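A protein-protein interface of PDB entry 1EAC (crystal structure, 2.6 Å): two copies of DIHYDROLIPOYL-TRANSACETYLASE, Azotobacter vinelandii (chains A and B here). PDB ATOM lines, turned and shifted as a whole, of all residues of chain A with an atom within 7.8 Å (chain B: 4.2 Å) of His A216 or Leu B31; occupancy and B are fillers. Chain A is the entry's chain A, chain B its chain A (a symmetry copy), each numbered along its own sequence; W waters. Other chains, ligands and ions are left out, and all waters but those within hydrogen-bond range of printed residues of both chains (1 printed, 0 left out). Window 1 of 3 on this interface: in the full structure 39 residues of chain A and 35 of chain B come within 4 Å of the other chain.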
ATOM      1  N   ASN A  37     -10.284  -1.736 -22.025  1.00  0.00           N
ATOM      2  CA  ASN A  37      -9.710  -0.608 -21.323  1.00  0.00           C
ATOM      3  C   ASN A  37      -9.917  -0.529 -19.824  1.00  0.00           C
ATOM      4  O   ASN A  37      -9.112   0.092 -19.111  1.00  0.00           O
ATOM      5  CB  ASN A  37     -10.238   0.672 -21.893  1.00  0.00           C
ATOM      6  CG  ASN A  37      -9.490   1.044 -23.131  1.00  0.00           C
ATOM      7  OD1 ASN A  37      -9.880   0.665 -24.203  1.00  0.00           O
ATOM      8  ND2 ASN A  37      -8.375   1.746 -23.083  1.00  0.00           N
ATOM      9  N   VAL A  38     -10.985  -1.136 -19.310  1.00  0.00           N
ATOM     10  CA  VAL A  38     -11.344  -0.990 -17.918  1.00  0.00           C
ATOM     11  C   VAL A  38     -10.996  -2.248 -17.131  1.00  0.00           C
ATOM     12  O   VAL A  38     -11.658  -3.272 -17.369  1.00  0.00           O
ATOM     13  CB  VAL A  38     -12.872  -0.635 -17.931  1.00  0.00           C
ATOM     14  CG1 VAL A  38     -13.340  -0.399 -16.530  1.00  0.00           C
ATOM     15  CG2 VAL A  38     -13.139   0.643 -18.675  1.00  0.00           C
ATOM     16  N   PRO A  39     -10.053  -2.321 -16.194  1.00  0.00           N
ATOM     17  CA  PRO A  39      -9.920  -3.491 -15.331  1.00  0.00           C
ATOM     18  C   PRO A  39     -11.107  -3.496 -14.359  1.00  0.00           C
ATOM     19  O   PRO A  39     -11.184  -2.671 -13.432  1.00  0.00           O
ATOM     20  CB  PRO A  39      -8.561  -3.314 -14.716  1.00  0.00           C
ATOM     21  CG  PRO A  39      -8.354  -1.838 -14.737  1.00  0.00           C
ATOM     22  CD  PRO A  39      -9.010  -1.344 -15.987  1.00  0.00           C
ATOM     23  N   HIS A  40     -12.053  -4.407 -14.673  1.00  0.00           N
ATOM     24  CA  HIS A  40     -13.382  -4.564 -14.033  1.00  0.00           C
ATOM     25  C   HIS A  40     -13.439  -5.310 -12.749  1.00  0.00           C
ATOM     26  O   HIS A  40     -12.861  -6.397 -12.709  1.00  0.00           O
ATOM     27  CB  HIS A  40     -14.461  -5.312 -14.905  1.00  0.00           C
ATOM     28  CG  HIS A  40     -14.964  -4.500 -16.112  1.00  0.00           C
ATOM     29  ND1 HIS A  40     -14.264  -4.131 -17.197  1.00  0.00           N
ATOM     30  CD2 HIS A  40     -16.228  -3.977 -16.259  1.00  0.00           C
ATOM     31  CE1 HIS A  40     -15.040  -3.423 -17.969  1.00  0.00           C
ATOM     32  NE2 HIS A  40     -16.220  -3.332 -17.407  1.00  0.00           N
ATOM     33  N   VAL A  41     -14.138  -4.809 -11.728  1.00  0.00           N
ATOM     34  CA  VAL A  41     -14.403  -5.614 -10.541  1.00  0.00           C
ATOM     35  C   VAL A  41     -15.890  -5.522 -10.259  1.00  0.00           C
ATOM     36  O   VAL A  41     -16.453  -4.491 -10.599  1.00  0.00           O
ATOM     37  CB  VAL A  41     -13.606  -5.085  -9.359  1.00  0.00           C
ATOM     38  CG1 VAL A  41     -13.927  -5.862  -8.088  1.00  0.00           C
ATOM     39  CG2 VAL A  41     -12.140  -5.276  -9.635  1.00  0.00           C
ATOM     40  N   VAL A 178     -18.931  -1.863 -17.454  1.00  0.00           N
ATOM     41  CA  VAL A 178     -18.837  -0.433 -17.294  1.00  0.00           C
ATOM     42  C   VAL A 178     -18.903   0.159 -18.655  1.00  0.00           C
ATOM     43  O   VAL A 178     -18.256  -0.258 -19.610  1.00  0.00           O
ATOM     44  CB  VAL A 178     -17.518  -0.041 -16.630  1.00  0.00           C
ATOM     45  CG1 VAL A 178     -17.295   1.453 -16.649  1.00  0.00           C
ATOM     46  CG2 VAL A 178     -17.589  -0.410 -15.184  1.00  0.00           C
ATOM     47  N   VAL A 183     -17.359   5.445 -14.826  1.00  0.00           N
ATOM     48  CA  VAL A 183     -16.509   4.646 -13.969  1.00  0.00           C
ATOM     49  C   VAL A 183     -17.223   3.569 -13.164  1.00  0.00           C
ATOM     50  O   VAL A 183     -16.536   2.787 -12.484  1.00  0.00           O
ATOM     51  CB  VAL A 183     -15.787   5.786 -13.223  1.00  0.00           C
ATOM     52  CG1 VAL A 183     -16.075   5.851 -11.781  1.00  0.00           C
ATOM     53  CG2 VAL A 183     -14.346   5.631 -13.557  1.00  0.00           C
ATOM     54  N   SER A 213     -20.432  -2.851 -10.848  1.00  0.00           N
ATOM     55  CA  SER A 213     -19.137  -3.039 -11.472  1.00  0.00           C
ATOM     56  C   SER A 213     -18.407  -1.697 -11.512  1.00  0.00           C
ATOM     57  O   SER A 213     -19.042  -0.662 -11.723  1.00  0.00           O
ATOM     58  CB  SER A 213     -19.288  -3.559 -12.877  1.00  0.00           C
ATOM     59  OG  SER A 213     -19.685  -4.915 -12.946  1.00  0.00           O
ATOM     60  N   TYR A 214     -17.090  -1.621 -11.319  1.00  0.00           N
ATOM     61  CA  TYR A 214     -16.384  -0.359 -11.344  1.00  0.00           C
ATOM     62  C   TYR A 214     -15.040  -0.470 -12.007  1.00  0.00           C
ATOM     63  O   TYR A 214     -14.520  -1.579 -12.196  1.00  0.00           O
ATOM     64  CB  TYR A 214     -16.172   0.154  -9.952  1.00  0.00           C
ATOM     65  CG  TYR A 214     -15.553  -0.794  -8.958  1.00  0.00           C
ATOM     66  CD1 TYR A 214     -16.317  -1.633  -8.193  1.00  0.00           C
ATOM     67  CD2 TYR A 214     -14.195  -0.793  -8.771  1.00  0.00           C
ATOM     68  CE1 TYR A 214     -15.704  -2.462  -7.238  1.00  0.00           C
ATOM     69  CE2 TYR A 214     -13.581  -1.611  -7.832  1.00  0.00           C
ATOM     70  CZ  TYR A 214     -14.327  -2.452  -7.056  1.00  0.00           C
ATOM     71  OH  TYR A 214     -13.687  -3.253  -6.111  1.00  0.00           O
ATOM     72  N   ASP A 215     -14.516   0.701 -12.368  1.00  0.00           N
ATOM     73  CA  ASP A 215     -13.235   0.814 -13.032  1.00  0.00           C
ATOM     74  C   ASP A 215     -12.211   0.866 -11.924  1.00  0.00           C
ATOM     75  O   ASP A 215     -11.944   1.919 -11.353  1.00  0.00           O
ATOM     76  CB  ASP A 215     -13.157   2.084 -13.821  1.00  0.00           C
ATOM     77  CG  ASP A 215     -11.886   2.226 -14.646  1.00  0.00           C
ATOM     78  OD1 ASP A 215     -10.870   1.562 -14.391  1.00  0.00           O
ATOM     79  OD2 ASP A 215     -11.935   3.032 -15.575  1.00  0.00           O
ATOM     80  N   HIS A 216     -11.517  -0.241 -11.691  1.00  0.00           N
ATOM     81  CA  HIS A 216     -10.641  -0.300 -10.544  1.00  0.00           C
ATOM     82  C   HIS A 216      -9.416   0.618 -10.630  1.00  0.00           C
ATOM     83  O   HIS A 216      -8.724   0.811  -9.636  1.00  0.00           O
ATOM     84  CB  HIS A 216     -10.247  -1.762 -10.356  1.00  0.00           C
ATOM     85  CG  HIS A 216      -9.633  -2.069  -8.991  1.00  0.00           C
ATOM     86  ND1 HIS A 216      -9.339  -1.249  -7.979  1.00  0.00           N
ATOM     87  CD2 HIS A 216      -9.256  -3.311  -8.589  1.00  0.00           C
ATOM     88  CE1 HIS A 216      -8.807  -1.919  -7.008  1.00  0.00           C
ATOM     89  NE2 HIS A 216      -8.760  -3.161  -7.381  1.00  0.00           N
ATOM     90  N   ARG A 217      -9.092   1.215 -11.783  1.00  0.00           N
ATOM     91  CA  ARG A 217      -8.006   2.179 -11.895  1.00  0.00           C
ATOM     92  C   ARG A 217      -8.312   3.437 -11.089  1.00  0.00           C
ATOM     93  O   ARG A 217      -7.446   4.109 -10.558  1.00  0.00           O
ATOM     94  CB  ARG A 217      -7.821   2.625 -13.331  1.00  0.00           C
ATOM     95  CG  ARG A 217      -7.434   1.475 -14.237  1.00  0.00           C
ATOM     96  CD  ARG A 217      -7.342   1.970 -15.645  1.00  0.00           C
ATOM     97  NE  ARG A 217      -8.638   2.412 -16.114  1.00  0.00           N
ATOM     98  CZ  ARG A 217      -8.779   2.890 -17.338  1.00  0.00           C
ATOM     99  NH1 ARG A 217      -7.712   2.968 -18.156  1.00  0.00           N
ATOM    100  NH2 ARG A 217      -9.986   3.279 -17.749  1.00  0.00           N
ATOM    101  N   VAL A 218      -9.590   3.743 -11.083  1.00  0.00           N
ATOM    102  CA  VAL A 218     -10.138   4.936 -10.528  1.00  0.00           C
ATOM    103  C   VAL A 218     -10.787   4.578  -9.197  1.00  0.00           C
ATOM    104  O   VAL A 218     -10.686   5.378  -8.276  1.00  0.00           O
ATOM    105  CB  VAL A 218     -11.166   5.467 -11.568  1.00  0.00           C
ATOM    106  CG1 VAL A 218     -11.799   6.745 -11.035  1.00  0.00           C
ATOM    107  CG2 VAL A 218     -10.509   5.682 -12.945  1.00  0.00           C
ATOM    108  N   ILE A 219     -11.508   3.464  -8.991  1.00  0.00           N
ATOM    109  CA  ILE A 219     -12.115   3.202  -7.688  1.00  0.00           C
ATOM    110  C   ILE A 219     -11.497   1.996  -7.052  1.00  0.00           C
ATOM    111  O   ILE A 219     -11.310   0.999  -7.726  1.00  0.00           O
ATOM    112  CB  ILE A 219     -13.638   3.026  -7.860  1.00  0.00           C
ATOM    113  CG1 ILE A 219     -14.162   4.426  -7.824  1.00  0.00           C
ATOM    114  CG2 ILE A 219     -14.359   2.318  -6.722  1.00  0.00           C
ATOM    115  CD1 ILE A 219     -15.130   4.634  -8.912  1.00  0.00           C
ATOM    116  N   ASN A 220     -11.067   2.067  -5.807  1.00  0.00           N
ATOM    117  CA  ASN A 220     -10.507   0.949  -5.070  1.00  0.00           C
ATOM    118  C   ASN A 220     -11.607   0.168  -4.392  1.00  0.00           C
ATOM    119  O   ASN A 220     -12.688   0.685  -4.114  1.00  0.00           O
ATOM    120  CB  ASN A 220      -9.536   1.416  -3.994  1.00  0.00           C
ATOM    121  CG  ASN A 220     -10.129   2.536  -3.098  1.00  0.00           C
ATOM    122  OD1 ASN A 220     -10.094   3.713  -3.486  1.00  0.00           O
ATOM    123  ND2 ASN A 220     -10.740   2.374  -1.920  1.00  0.00           N
ATOM    124  N   GLY A 221     -11.248  -1.027  -3.976  1.00  0.00           N
ATOM    125  CA  GLY A 221     -12.198  -1.947  -3.419  1.00  0.00           C
ATOM    126  C   GLY A 221     -12.907  -1.389  -2.224  1.00  0.00           C
ATOM    127  O   GLY A 221     -14.124  -1.491  -2.106  1.00  0.00           O
ATOM    128  N   ALA A 222     -12.233  -0.724  -1.301  1.00  0.00           N
ATOM    129  CA  ALA A 222     -12.993  -0.193  -0.176  1.00  0.00           C
ATOM    130  C   ALA A 222     -13.914   0.932  -0.566  1.00  0.00           C
ATOM    131  O   ALA A 222     -14.978   1.007   0.019  1.00  0.00           O
ATOM    132  CB  ALA A 222     -12.132   0.357   0.880  1.00  0.00           C
ATOM    133  N   GLY B  27      -0.649   2.100  -9.517  1.00  0.00           N
ATOM    134  CA  GLY B  27      -1.745   1.182  -9.285  1.00  0.00           C
ATOM    135  C   GLY B  27      -2.566   0.961 -10.533  1.00  0.00           C
ATOM    136  O   GLY B  27      -2.783  -0.188 -10.928  1.00  0.00           O
ATOM    137  N   ALA B  28      -2.959   2.023 -11.219  1.00  0.00           N
ATOM    138  CA  ALA B  28      -3.747   1.914 -12.427  1.00  0.00           C
ATOM    139  C   ALA B  28      -3.026   1.083 -13.478  1.00  0.00           C
ATOM    140  O   ALA B  28      -3.613   0.139 -14.002  1.00  0.00           O
ATOM    141  CB  ALA B  28      -4.028   3.294 -12.991  1.00  0.00           C
ATOM    142  N   THR B  29      -1.743   1.311 -13.727  1.00  0.00           N
ATOM    143  CA  THR B  29      -0.961   0.569 -14.708  1.00  0.00           C
ATOM    144  C   THR B  29      -0.840  -0.931 -14.476  1.00  0.00           C
ATOM    145  O   THR B  29      -0.991  -1.758 -15.397  1.00  0.00           O
ATOM    146  CB  THR B  29       0.414   1.265 -14.742  1.00  0.00           C
ATOM    147  OG1 THR B  29       0.129   2.540 -15.323  1.00  0.00           O
ATOM    148  CG2 THR B  29       1.506   0.538 -15.521  1.00  0.00           C
ATOM    149  N   ASN B  30      -0.579  -1.263 -13.220  1.00  0.00           N
ATOM    150  CA  ASN B  30      -0.446  -2.643 -12.868  1.00  0.00           C
ATOM    151  C   ASN B  30      -1.741  -3.376 -13.008  1.00  0.00           C
ATOM    152  O   ASN B  30      -1.693  -4.536 -13.423  1.00  0.00           O
ATOM    153  CB  ASN B  30      -0.047  -2.881 -11.455  1.00  0.00           C
ATOM    154  CG  ASN B  30       1.325  -2.357 -11.114  1.00  0.00           C
ATOM    155  OD1 ASN B  30       2.231  -2.114 -11.925  1.00  0.00           O
ATOM    156  ND2 ASN B  30       1.462  -2.147  -9.819  1.00  0.00           N
ATOM    157  N   LEU B  31      -2.902  -2.776 -12.687  1.00  0.00           N
ATOM    158  CA  LEU B  31      -4.150  -3.511 -12.787  1.00  0.00           C
ATOM    159  C   LEU B  31      -4.516  -3.809 -14.215  1.00  0.00           C
ATOM    160  O   LEU B  31      -5.011  -4.887 -14.552  1.00  0.00           O
ATOM    161  CB  LEU B  31      -5.258  -2.737 -12.173  1.00  0.00           C
ATOM    162  CG  LEU B  31      -5.047  -2.533 -10.717  1.00  0.00           C
ATOM    163  CD1 LEU B  31      -5.944  -1.397 -10.344  1.00  0.00           C
ATOM    164  CD2 LEU B  31      -5.284  -3.793  -9.923  1.00  0.00           C
ATOM    165  N   HIS B  32      -4.250  -2.829 -15.060  1.00  0.00           N
ATOM    166  CA  HIS B  32      -4.546  -2.977 -16.441  1.00  0.00           C
ATOM    167  C   HIS B  32      -3.634  -4.026 -17.027  1.00  0.00           C
ATOM    168  O   HIS B  32      -4.136  -4.826 -17.816  1.00  0.00           O
ATOM    169  CB  HIS B  32      -4.369  -1.651 -17.111  1.00  0.00           C
ATOM    170  CG  HIS B  32      -5.166  -1.557 -18.399  1.00  0.00           C
ATOM    171  ND1 HIS B  32      -5.949  -2.471 -18.991  1.00  0.00           N
ATOM    172  CD2 HIS B  32      -5.194  -0.445 -19.196  1.00  0.00           C
ATOM    173  CE1 HIS B  32      -6.443  -1.974 -20.090  1.00  0.00           C
ATOM    174  NE2 HIS B  32      -5.980  -0.761 -20.199  1.00  0.00           N
ATOM    175  N   ARG B  33      -2.356  -4.078 -16.659  1.00  0.00           N
ATOM    176  CA  ARG B  33      -1.440  -5.107 -17.110  1.00  0.00           C
ATOM    177  C   ARG B  33      -1.941  -6.500 -16.720  1.00  0.00           C
ATOM    178  O   ARG B  33      -1.997  -7.392 -17.579  1.00  0.00           O
ATOM    179  CB  ARG B  33      -0.129  -4.832 -16.482  1.00  0.00           C
ATOM    180  CG  ARG B  33       0.997  -5.059 -17.421  1.00  0.00           C
ATOM    181  CD  ARG B  33       2.151  -5.585 -16.601  1.00  0.00           C
ATOM    182  NE  ARG B  33       2.617  -4.719 -15.522  1.00  0.00           N
ATOM    183  CZ  ARG B  33       3.426  -3.681 -15.799  1.00  0.00           C
ATOM    184  NH1 ARG B  33       3.832  -3.405 -17.073  1.00  0.00           N
ATOM    185  NH2 ARG B  33       3.836  -2.916 -14.778  1.00  0.00           N
ATOM    186  N   SER B  34      -2.370  -6.722 -15.456  1.00  0.00           N
ATOM    187  CA  SER B  34      -2.968  -7.978 -15.037  1.00  0.00           C
ATOM    188  C   SER B  34      -4.244  -8.282 -15.750  1.00  0.00           C
ATOM    189  O   SER B  34      -4.458  -9.442 -16.093  1.00  0.00           O
ATOM    190  CB  SER B  34      -3.379  -8.046 -13.604  1.00  0.00           C
ATOM    191  OG  SER B  34      -2.206  -7.783 -12.863  1.00  0.00           O
ATOM    192  N   TRP B  35      -5.129  -7.310 -15.947  1.00  0.00           N
ATOM    193  CA  TRP B  35      -6.406  -7.528 -16.576  1.00  0.00           C
ATOM    194  C   TRP B  35      -6.252  -8.118 -17.969  1.00  0.00           C
ATOM    195  O   TRP B  35      -6.962  -9.056 -18.344  1.00  0.00           O
ATOM    196  CB  TRP B  35      -7.104  -6.202 -16.621  1.00  0.00           C
ATOM    197  CG  TRP B  35      -8.491  -6.241 -17.207  1.00  0.00           C
ATOM    198  CD1 TRP B  35      -8.800  -5.680 -18.415  1.00  0.00           C
ATOM    199  CD2 TRP B  35      -9.556  -6.888 -16.645  1.00  0.00           C
ATOM    200  NE1 TRP B  35     -10.069  -5.991 -18.632  1.00  0.00           N
ATOM    201  CE2 TRP B  35     -10.544  -6.706 -17.606  1.00  0.00           C
ATOM    202  CE3 TRP B  35      -9.782  -7.579 -15.477  1.00  0.00           C
ATOM    203  CZ2 TRP B  35     -11.790  -7.223 -17.420  1.00  0.00           C
ATOM    204  CZ3 TRP B  35     -11.028  -8.084 -15.298  1.00  0.00           C
ATOM    205  CH2 TRP B  35     -12.008  -7.907 -16.254  1.00  0.00           C
HETATM  206  O   HOH W   1      -4.899   3.158  -8.972  1.00  0.00           O
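NE2 of His B32 is in hydrogen-bond range of O of Asn A37 (3.4 Å).
The indole nitrogen of Trp B35 sits at hydrogen-bond distance from the backbone carbonyl oxygen of Val A38, 3.4 Å away.
The guanidinium group (NH2) of Arg A217 is in salt-bridge range of the side-chain carboxylate (OD2) of Asp A215 (2.9 Å).
A ring nitrogen (NE2) of His A40 is in hydrogen-bond range of the backbone NH (N) of Val A178 (3.1 Å).
O of Ile A219 is in hydrogen-bond range of ND1 of His A216.
The backbone carbonyl oxygen (O) of Asn A37 lies close to the guanidinium group (NH1) of Arg A217 (3.3 Å).
The backbone carbonyl oxygen (O) of Pro A39 sits at hydrogen-bond distance from the backbone NH (N) of His A216 (3.0 Å).
O of Val A38 lies within hydrogen-bond range of ND1 of His A40 (2.7 Å).
Among the printed residues, pairs that only touch across the chains: Pro A39 with Leu B31, Pro A39 with Trp B35, His A40 with Trp B35, His A216 with Leu B31 and Arg A217 with Ala B28.
Printed residues of chain B within 4 Å of Asn A37: His B32.
Of the printed residues of chain B, Val A38 touches Trp B35 (3.4 Å).
His A216 touches just one residue of chain B: Leu B31 (3.6 Å).
Asn A220 touches none of the printed residues of chain B.
Ala A222 touches none of the printed residues of chain B.
Printed residues of chain A within 4 Å of Ala B28: Arg A217 (3.9 Å).
Of chain A, only Pro A39 and His A216 come within 4 Å of Leu B31.
The nearest printed residue of chain A that does not touch His B32 is Pro A39 (4.2 Å).
Of the 9 printed residues of chain B, 4 touch a printed residue of chain A.
Of the 17 printed residues of chain A, 6 touch a printed residue of chain B.
Printed residues of chain A that touch a printed residue of chain B: Asn A37, Val A38, Pro A39, His A40, His A216 and Arg A217.
Hydrophobic or aromatic side chains of chain A within 4 Å of the printed part of chain B: Pro A39, His A40 and His A216.
Among the printed residues, 7 pairs touch across the chains.
Among the printed residues, no Asp or Glu carboxylate lies within 4 Å of a Lys or Arg side-chain nitrogen of the other chain.
No position is printed for both chains.
Of the 7 pairs that touch across the chains among the printed residues, none has its exchanged pair printed and touching as well.
Water W1 bridges O of Arg A217 (3.1 Å) and N of Ala B28 (3.2 Å).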
